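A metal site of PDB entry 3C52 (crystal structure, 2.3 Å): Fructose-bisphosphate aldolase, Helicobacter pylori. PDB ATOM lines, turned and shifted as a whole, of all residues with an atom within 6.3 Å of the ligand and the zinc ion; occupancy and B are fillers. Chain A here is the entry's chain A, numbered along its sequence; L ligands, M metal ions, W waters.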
ATOM      1  N   ALA A  21      27.161  14.904 -26.514  1.00  0.00           N
ATOM      2  CA  ALA A  21      27.040  14.894 -25.073  1.00  0.00           C
ATOM      3  C   ALA A  21      25.748  15.650 -24.807  1.00  0.00           C
ATOM      4  O   ALA A  21      25.651  16.855 -25.068  1.00  0.00           O
ATOM      5  CB  ALA A  21      28.191  15.589 -24.421  1.00  0.00           C
ATOM      6  N   ASN A  23      22.664  16.910 -22.392  1.00  0.00           N
ATOM      7  CA  ASN A  23      22.272  17.258 -21.035  1.00  0.00           C
ATOM      8  C   ASN A  23      20.861  16.841 -20.724  1.00  0.00           C
ATOM      9  O   ASN A  23      20.006  16.830 -21.610  1.00  0.00           O
ATOM     10  CB  ASN A  23      22.390  18.756 -20.821  1.00  0.00           C
ATOM     11  CG  ASN A  23      23.802  19.219 -20.718  1.00  0.00           C
ATOM     12  OD1 ASN A  23      24.528  19.246 -21.707  1.00  0.00           O
ATOM     13  ND2 ASN A  23      24.212  19.598 -19.511  1.00  0.00           N
ATOM     14  N   GLN A  47      25.044  13.898 -19.884  1.00  0.00           N
ATOM     15  CA  GLN A  47      25.594  14.834 -18.915  1.00  0.00           C
ATOM     16  C   GLN A  47      24.614  15.744 -18.158  1.00  0.00           C
ATOM     17  O   GLN A  47      23.584  16.186 -18.688  1.00  0.00           O
ATOM     18  CB  GLN A  47      26.730  15.653 -19.530  1.00  0.00           C
ATOM     19  CG  GLN A  47      26.392  16.390 -20.784  1.00  0.00           C
ATOM     20  CD  GLN A  47      27.571  17.199 -21.278  1.00  0.00           C
ATOM     21  OE1 GLN A  47      28.719  16.753 -21.196  1.00  0.00           O
ATOM     22  NE2 GLN A  47      27.305  18.385 -21.802  1.00  0.00           N
ATOM     23  N   ASP A  82      29.038  18.026 -16.006  1.00  0.00           N
ATOM     24  CA  ASP A  82      29.249  19.080 -16.959  1.00  0.00           C
ATOM     25  C   ASP A  82      29.557  20.350 -16.194  1.00  0.00           C
ATOM     26  O   ASP A  82      28.819  20.704 -15.281  1.00  0.00           O
ATOM     27  CB  ASP A  82      27.987  19.247 -17.792  1.00  0.00           C
ATOM     28  CG  ASP A  82      28.154  20.224 -18.929  1.00  0.00           C
ATOM     29  OD1 ASP A  82      29.306  20.482 -19.326  1.00  0.00           O
ATOM     30  OD2 ASP A  82      27.133  20.747 -19.416  1.00  0.00           O
ATOM     31  N   HIS A  83      30.662  20.990 -16.556  1.00  0.00           N
ATOM     32  CA  HIS A  83      31.163  22.179 -15.851  1.00  0.00           C
ATOM     33  C   HIS A  83      31.211  22.035 -14.325  1.00  0.00           C
ATOM     34  O   HIS A  83      30.530  22.759 -13.612  1.00  0.00           O
ATOM     35  CB  HIS A  83      30.367  23.426 -16.228  1.00  0.00           C
ATOM     36  CG  HIS A  83      30.526  23.799 -17.669  1.00  0.00           C
ATOM     37  ND1 HIS A  83      31.544  24.601 -18.110  1.00  0.00           N
ATOM     38  CD2 HIS A  83      29.802  23.477 -18.770  1.00  0.00           C
ATOM     39  CE1 HIS A  83      31.449  24.770 -19.418  1.00  0.00           C
ATOM     40  NE2 HIS A  83      30.399  24.084 -19.839  1.00  0.00           N
ATOM     41  N   MET A 102      33.856  16.903 -15.598  1.00  0.00           N
ATOM     42  CA  MET A 102      34.620  18.010 -16.163  1.00  0.00           C
ATOM     43  C   MET A 102      34.947  18.973 -15.034  1.00  0.00           C
ATOM     44  O   MET A 102      34.070  19.312 -14.223  1.00  0.00           O
ATOM     45  CB  MET A 102      33.873  18.747 -17.261  1.00  0.00           C
ATOM     46  CG  MET A 102      34.599  19.994 -17.696  1.00  0.00           C
ATOM     47  SD  MET A 102      33.516  21.175 -18.503  1.00  0.00           S
ATOM     48  CE  MET A 102      34.722  22.239 -19.298  1.00  0.00           C
ATOM     49  N   GLU A 134      39.162  22.469 -19.409  1.00  0.00           N
ATOM     50  CA  GLU A 134      39.042  23.465 -20.468  1.00  0.00           C
ATOM     51  C   GLU A 134      40.225  24.409 -20.510  1.00  0.00           C
ATOM     52  O   GLU A 134      40.826  24.728 -19.485  1.00  0.00           O
ATOM     53  CB  GLU A 134      37.747  24.262 -20.311  1.00  0.00           C
ATOM     54  CG  GLU A 134      37.568  25.360 -21.355  1.00  0.00           C
ATOM     55  CD  GLU A 134      36.222  26.049 -21.289  1.00  0.00           C
ATOM     56  OE1 GLU A 134      35.318  25.513 -20.616  1.00  0.00           O
ATOM     57  OE2 GLU A 134      36.067  27.126 -21.903  1.00  0.00           O
ATOM     58  N   LEU A 138      34.906  30.554 -23.277  1.00  0.00           N
ATOM     59  CA  LEU A 138      33.848  30.440 -24.282  1.00  0.00           C
ATOM     60  C   LEU A 138      33.184  31.751 -24.696  1.00  0.00           C
ATOM     61  O   LEU A 138      32.093  32.083 -24.245  1.00  0.00           O
ATOM     62  CB  LEU A 138      32.798  29.418 -23.825  1.00  0.00           C
ATOM     63  CG  LEU A 138      33.278  27.972 -23.825  1.00  0.00           C
ATOM     64  CD1 LEU A 138      32.376  27.085 -22.986  1.00  0.00           C
ATOM     65  CD2 LEU A 138      33.395  27.445 -25.242  1.00  0.00           C
ATOM     66  N   SER A 179      30.250  29.565 -27.875  1.00  0.00           N
ATOM     67  CA  SER A 179      29.789  29.947 -26.542  1.00  0.00           C
ATOM     68  C   SER A 179      28.451  29.280 -26.296  1.00  0.00           C
ATOM     69  O   SER A 179      27.765  28.912 -27.264  1.00  0.00           O
ATOM     70  CB  SER A 179      29.666  31.467 -26.415  1.00  0.00           C
ATOM     71  OG  SER A 179      28.829  31.999 -27.427  1.00  0.00           O
ATOM     72  N   HIS A 180      28.087  29.127 -25.027  1.00  0.00           N
ATOM     73  CA  HIS A 180      26.824  28.481 -24.662  1.00  0.00           C
ATOM     74  C   HIS A 180      25.602  29.333 -25.032  1.00  0.00           C
ATOM     75  O   HIS A 180      25.727  30.551 -25.190  1.00  0.00           O
ATOM     76  CB  HIS A 180      26.819  28.161 -23.158  1.00  0.00           C
ATOM     77  CG  HIS A 180      27.951  27.292 -22.715  1.00  0.00           C
ATOM     78  ND1 HIS A 180      28.589  27.449 -21.508  1.00  0.00           N
ATOM     79  CD2 HIS A 180      28.579  26.268 -23.346  1.00  0.00           C
ATOM     80  CE1 HIS A 180      29.551  26.552 -21.394  1.00  0.00           C
ATOM     81  NE2 HIS A 180      29.568  25.822 -22.496  1.00  0.00           N
ATOM     82  N   GLY A 181      24.447  28.689 -25.164  1.00  0.00           N
ATOM     83  CA  GLY A 181      23.217  29.413 -25.426  1.00  0.00           C
ATOM     84  C   GLY A 181      22.814  29.591 -26.885  1.00  0.00           C
ATOM     85  O   GLY A 181      23.545  29.216 -27.807  1.00  0.00           O
ATOM     86  N   ALA A 182      21.632  30.172 -27.086  1.00  0.00           N
ATOM     87  CA  ALA A 182      21.023  30.281 -28.410  1.00  0.00           C
ATOM     88  C   ALA A 182      21.620  31.377 -29.280  1.00  0.00           C
ATOM     89  O   ALA A 182      21.312  31.475 -30.474  1.00  0.00           O
ATOM     90  CB  ALA A 182      19.517  30.467 -28.271  1.00  0.00           C
ATOM     91  N   LYS A 184      25.116  32.453 -30.302  1.00  0.00           N
ATOM     92  CA  LYS A 184      26.551  32.181 -30.304  1.00  0.00           C
ATOM     93  C   LYS A 184      27.368  33.144 -31.192  1.00  0.00           C
ATOM     94  O   LYS A 184      28.445  33.604 -30.785  1.00  0.00           O
ATOM     95  CB  LYS A 184      26.826  30.740 -30.744  1.00  0.00           C
ATOM     96  CG  LYS A 184      26.159  29.713 -29.837  1.00  0.00           C
ATOM     97  CD  LYS A 184      26.387  28.305 -30.328  1.00  0.00           C
ATOM     98  CE  LYS A 184      25.445  27.344 -29.603  1.00  0.00           C
ATOM     99  NZ  LYS A 184      25.563  27.513 -28.133  1.00  0.00           N
ATOM    100  N   LEU A 209      33.841  19.869 -27.788  1.00  0.00           N
ATOM    101  CA  LEU A 209      33.325  21.142 -28.271  1.00  0.00           C
ATOM    102  C   LEU A 209      32.134  21.577 -27.428  1.00  0.00           C
ATOM    103  O   LEU A 209      31.072  20.918 -27.432  1.00  0.00           O
ATOM    104  CB  LEU A 209      32.931  21.088 -29.738  1.00  0.00           C
ATOM    105  CG  LEU A 209      32.449  22.432 -30.296  1.00  0.00           C
ATOM    106  CD1 LEU A 209      33.623  23.401 -30.473  1.00  0.00           C
ATOM    107  CD2 LEU A 209      31.723  22.263 -31.615  1.00  0.00           C
ATOM    108  N   HIS A 210      32.308  22.672 -26.685  1.00  0.00           N
ATOM    109  CA  HIS A 210      31.235  23.241 -25.898  1.00  0.00           C
ATOM    110  C   HIS A 210      30.473  24.233 -26.727  1.00  0.00           C
ATOM    111  O   HIS A 210      30.969  24.712 -27.747  1.00  0.00           O
ATOM    112  CB  HIS A 210      31.794  23.935 -24.666  1.00  0.00           C
ATOM    113  CG  HIS A 210      32.143  22.994 -23.557  1.00  0.00           C
ATOM    114  ND1 HIS A 210      31.453  22.973 -22.361  1.00  0.00           N
ATOM    115  CD2 HIS A 210      33.068  22.019 -23.471  1.00  0.00           C
ATOM    116  CE1 HIS A 210      31.963  22.042 -21.582  1.00  0.00           C
ATOM    117  NE2 HIS A 210      32.938  21.444 -22.240  1.00  0.00           N
ATOM    118  N   GLY A 211      29.265  24.552 -26.262  1.00  0.00           N
ATOM    119  CA  GLY A 211      28.418  25.511 -26.937  1.00  0.00           C
ATOM    120  C   GLY A 211      28.149  25.096 -28.369  1.00  0.00           C
ATOM    121  O   GLY A 211      28.120  25.933 -29.278  1.00  0.00           O
ATOM    122  N   ALA A 212      27.919  23.795 -28.550  1.00  0.00           N
ATOM    123  CA  ALA A 212      27.815  23.188 -29.882  1.00  0.00           C
ATOM    124  C   ALA A 212      26.403  22.987 -30.430  1.00  0.00           C
ATOM    125  O   ALA A 212      26.225  22.270 -31.404  1.00  0.00           O
ATOM    126  CB  ALA A 212      28.566  21.871 -29.909  1.00  0.00           C
ATOM    127  N   SER A 213      25.400  23.607 -29.819  1.00  0.00           N
ATOM    128  CA  SER A 213      24.060  23.493 -30.386  1.00  0.00           C
ATOM    129  C   SER A 213      24.040  24.160 -31.751  1.00  0.00           C
ATOM    130  O   SER A 213      24.830  25.068 -32.024  1.00  0.00           O
ATOM    131  CB  SER A 213      22.986  24.076 -29.476  1.00  0.00           C
ATOM    132  OG  SER A 213      22.606  23.128 -28.494  1.00  0.00           O
ATOM    133  N   ALA A 214      23.130  23.687 -32.607  1.00  0.00           N
ATOM    134  CA  ALA A 214      23.111  24.065 -34.001  1.00  0.00           C
ATOM    135  C   ALA A 214      21.974  25.045 -34.262  1.00  0.00           C
ATOM    136  O   ALA A 214      22.084  25.928 -35.125  1.00  0.00           O
ATOM    137  CB  ALA A 214      22.945  22.833 -34.859  1.00  0.00           C
ATOM    138  N   ASN A 253      29.087  18.922 -27.035  1.00  0.00           N
ATOM    139  CA  ASN A 253      28.097  19.247 -26.006  1.00  0.00           C
ATOM    140  C   ASN A 253      26.856  19.906 -26.584  1.00  0.00           C
ATOM    141  O   ASN A 253      26.947  20.928 -27.271  1.00  0.00           O
ATOM    142  CB  ASN A 253      28.703  20.162 -24.947  1.00  0.00           C
ATOM    143  CG  ASN A 253      29.803  19.485 -24.168  1.00  0.00           C
ATOM    144  OD1 ASN A 253      30.200  18.370 -24.466  1.00  0.00           O
ATOM    145  ND2 ASN A 253      30.301  20.163 -23.156  1.00  0.00           N
ATOM    146  N   THR A 254      25.698  19.322 -26.298  1.00  0.00           N
ATOM    147  CA  THR A 254      24.451  19.742 -26.902  1.00  0.00           C
ATOM    148  C   THR A 254      23.369  19.846 -25.836  1.00  0.00           C
ATOM    149  O   THR A 254      23.054  18.864 -25.178  1.00  0.00           O
ATOM    150  CB  THR A 254      24.005  18.699 -27.949  1.00  0.00           C
ATOM    151  OG1 THR A 254      25.146  18.240 -28.685  1.00  0.00           O
ATOM    152  CG2 THR A 254      22.983  19.285 -28.909  1.00  0.00           C
ATOM    153  N   ASP A 255      22.795  21.019 -25.658  1.00  0.00           N
ATOM    154  CA  ASP A 255      21.810  21.220 -24.598  1.00  0.00           C
ATOM    155  C   ASP A 255      20.673  22.140 -25.060  1.00  0.00           C
ATOM    156  O   ASP A 255      19.515  21.741 -25.099  1.00  0.00           O
ATOM    157  CB  ASP A 255      22.479  21.772 -23.349  1.00  0.00           C
ATOM    158  CG  ASP A 255      21.517  21.939 -22.211  1.00  0.00           C
ATOM    159  OD1 ASP A 255      20.355  21.490 -22.336  1.00  0.00           O
ATOM    160  OD2 ASP A 255      21.933  22.521 -21.185  1.00  0.00           O
ATOM    161  N   THR A 256      21.020  23.375 -25.418  1.00  0.00           N
ATOM    162  CA  THR A 256      20.040  24.344 -25.900  1.00  0.00           C
ATOM    163  C   THR A 256      19.080  23.772 -26.948  1.00  0.00           C
ATOM    164  O   THR A 256      17.873  24.064 -26.933  1.00  0.00           O
ATOM    165  CB  THR A 256      20.774  25.564 -26.510  1.00  0.00           C
ATOM    166  OG1 THR A 256      21.470  26.265 -25.471  1.00  0.00           O
ATOM    167  CG2 THR A 256      19.777  26.496 -27.181  1.00  0.00           C
ATOM    168  N   ASP A 257      19.596  22.985 -27.872  1.00  0.00           N
ATOM    169  CA  ASP A 257      18.773  22.421 -28.945  1.00  0.00           C
ATOM    170  C   ASP A 257      17.650  21.539 -28.388  1.00  0.00           C
ATOM    171  O   ASP A 257      16.519  21.612 -28.855  1.00  0.00           O
ATOM    172  CB  ASP A 257      19.628  21.641 -29.936  1.00  0.00           C
ATOM    173  CG  ASP A 257      20.213  22.537 -31.034  1.00  0.00           C
ATOM    174  OD1 ASP A 257      19.891  23.748 -31.050  1.00  0.00           O
ATOM    175  OD2 ASP A 257      20.987  22.025 -31.874  1.00  0.00           O
ATOM    176  N   ARG A 259      16.309  21.601 -25.264  1.00  0.00           N
ATOM    177  CA  ARG A 259      15.383  22.427 -24.485  1.00  0.00           C
ATOM    178  C   ARG A 259      14.401  23.204 -25.359  1.00  0.00           C
ATOM    179  O   ARG A 259      13.204  23.266 -25.065  1.00  0.00           O
ATOM    180  CB  ARG A 259      16.170  23.376 -23.572  1.00  0.00           C
ATOM    181  CG  ARG A 259      16.952  22.660 -22.480  1.00  0.00           C
ATOM    182  CD  ARG A 259      18.282  23.328 -22.150  1.00  0.00           C
ATOM    183  NE  ARG A 259      18.170  24.615 -21.465  1.00  0.00           N
ATOM    184  CZ  ARG A 259      19.172  25.167 -20.783  1.00  0.00           C
ATOM    185  NH1 ARG A 259      20.338  24.565 -20.698  1.00  0.00           N
ATOM    186  NH2 ARG A 259      19.007  26.340 -20.173  1.00  0.00           N
HETATM  187  C1  LIG L   1      27.371  22.884 -23.630  1.00  0.00           C
HETATM  188  C2  LIG L   1      26.008  23.112 -24.284  1.00  0.00           C
HETATM  189  N1  LIG L   1      27.511  21.906 -22.562  1.00  0.00           N
HETATM  190  O1  LIG L   1      28.279  22.207 -21.431  1.00  0.00           O
HETATM  191  O2  LIG L   1      28.322  23.504 -23.992  1.00  0.00           O
HETATM  192  O3  LIG L   1      26.114  24.138 -25.239  1.00  0.00           O
HETATM  193  O4  LIG L   1      25.172  25.138 -27.571  1.00  0.00           O
HETATM  194  O5  LIG L   1      23.676  23.411 -26.136  1.00  0.00           O
HETATM  195  O6  LIG L   1      24.158  25.780 -25.327  1.00  0.00           O
HETATM  196  P1  LIG L   1      24.758  24.653 -26.043  1.00  0.00           P
HETATM  197 ZN    ZN M   1      29.645  23.904 -21.663  1.00  0.00          ZN
HETATM  198  O   HOH W   1      24.165  25.585 -22.742  1.00  0.00           O
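An oxygen (O4) of the ligand lies within salt-bridge range of the side-chain amino group (NZ) of Lys 184.
The backbone NH (N) of Asp 255 lies within hydrogen-bond range of an oxygen (O5) of the ligand, 2.6 Å away.
N of Ser 213 is in hydrogen-bond range of O4 of the ligand.
An oxygen (O5) of the ligand sits at hydrogen-bond distance from the side-chain hydroxyl of Ser 213 (2.6 Å).
An oxygen (O2) of the ligand is in hydrogen-bond range of the backbone NH of Gly 211, 2.7 Å away.
N of Thr 256 lies within hydrogen-bond range of O5 of the ligand (2.8 Å).
OG1 of Thr 256 is in hydrogen-bond range of O6 of the ligand (2.7 Å).
The side-chain carboxylate of Asp 82 sits at hydrogen-bond distance from a nitrogen (N1) of the ligand (3.4 Å).
N of Gly 181 sits at hydrogen-bond distance from O6 of the ligand (2.9 Å).
ND2 of Asn 253 sits close to N1 of the ligand.
The backbone NH (N) of Ala 212 is in hydrogen-bond range of an oxygen (O4) of the ligand, 3.2 Å away.
A ring nitrogen (NE2) of His 210 lies close to the side-chain amide nitrogen (ND2) of Asn 253 (3.1 Å).
SD of Met 102 lies close to NE2 of His 210, at 3.8 Å.
The side-chain amino group (NZ) of Lys 184 sits close to the backbone carbonyl oxygen (O) of Gly 211 (3.2 Å).
The side-chain amino group of Lys 184 sits at hydrogen-bond distance from the backbone carbonyl oxygen of Gly 181 (2.7 Å).
The backbone NH (N) of Thr 256 lies within hydrogen-bond range of the side-chain hydroxyl (OG) of Ser 213, at 3.5 Å.
The side-chain carboxylate of Asp 82 is in hydrogen-bond range of the side-chain amide nitrogen of Gln 47 (3.4 Å).
The backbone NH (N) of Asn 253 lies within hydrogen-bond range of the backbone carbonyl oxygen (O) of Leu 209 (2.8 Å).
The backbone NH (N) of Thr 254 lies within hydrogen-bond range of the backbone carbonyl oxygen (O) of Ala 21 (2.8 Å).
Merely in contact with the ligand: Thr 254 (3.6 Å) and Gln 47 (3.6 Å).
Hydrophobic or aromatic side chains within 4 Å of the ligand: His 83, His 180 and His 210.
Of the 25 residues printed, 14 come within 4 Å of the ligand.
Along chain A the residues within 4 Å of the ligand span positions 47 to 256.
Within 4 Å of the zinc ion: His 83, His 180 and His 210.
Along chain A the residues within 4 Å of the zinc ion span positions 83 to 210.
A ring nitrogen (NE2) of His 83 is bound to the zinc ion, at 2.0 Å.
The zinc ion is bound by a ring nitrogen (NE2) of His 180.
A ring nitrogen (ND1) of His 210 binds the zinc ion (2.2 Å).
The zinc ion is bound by an oxygen (O1) of the ligand, 2.2 Å away.
Slightly farther from the zinc ion lies O2 of the ligand (2.7 Å).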
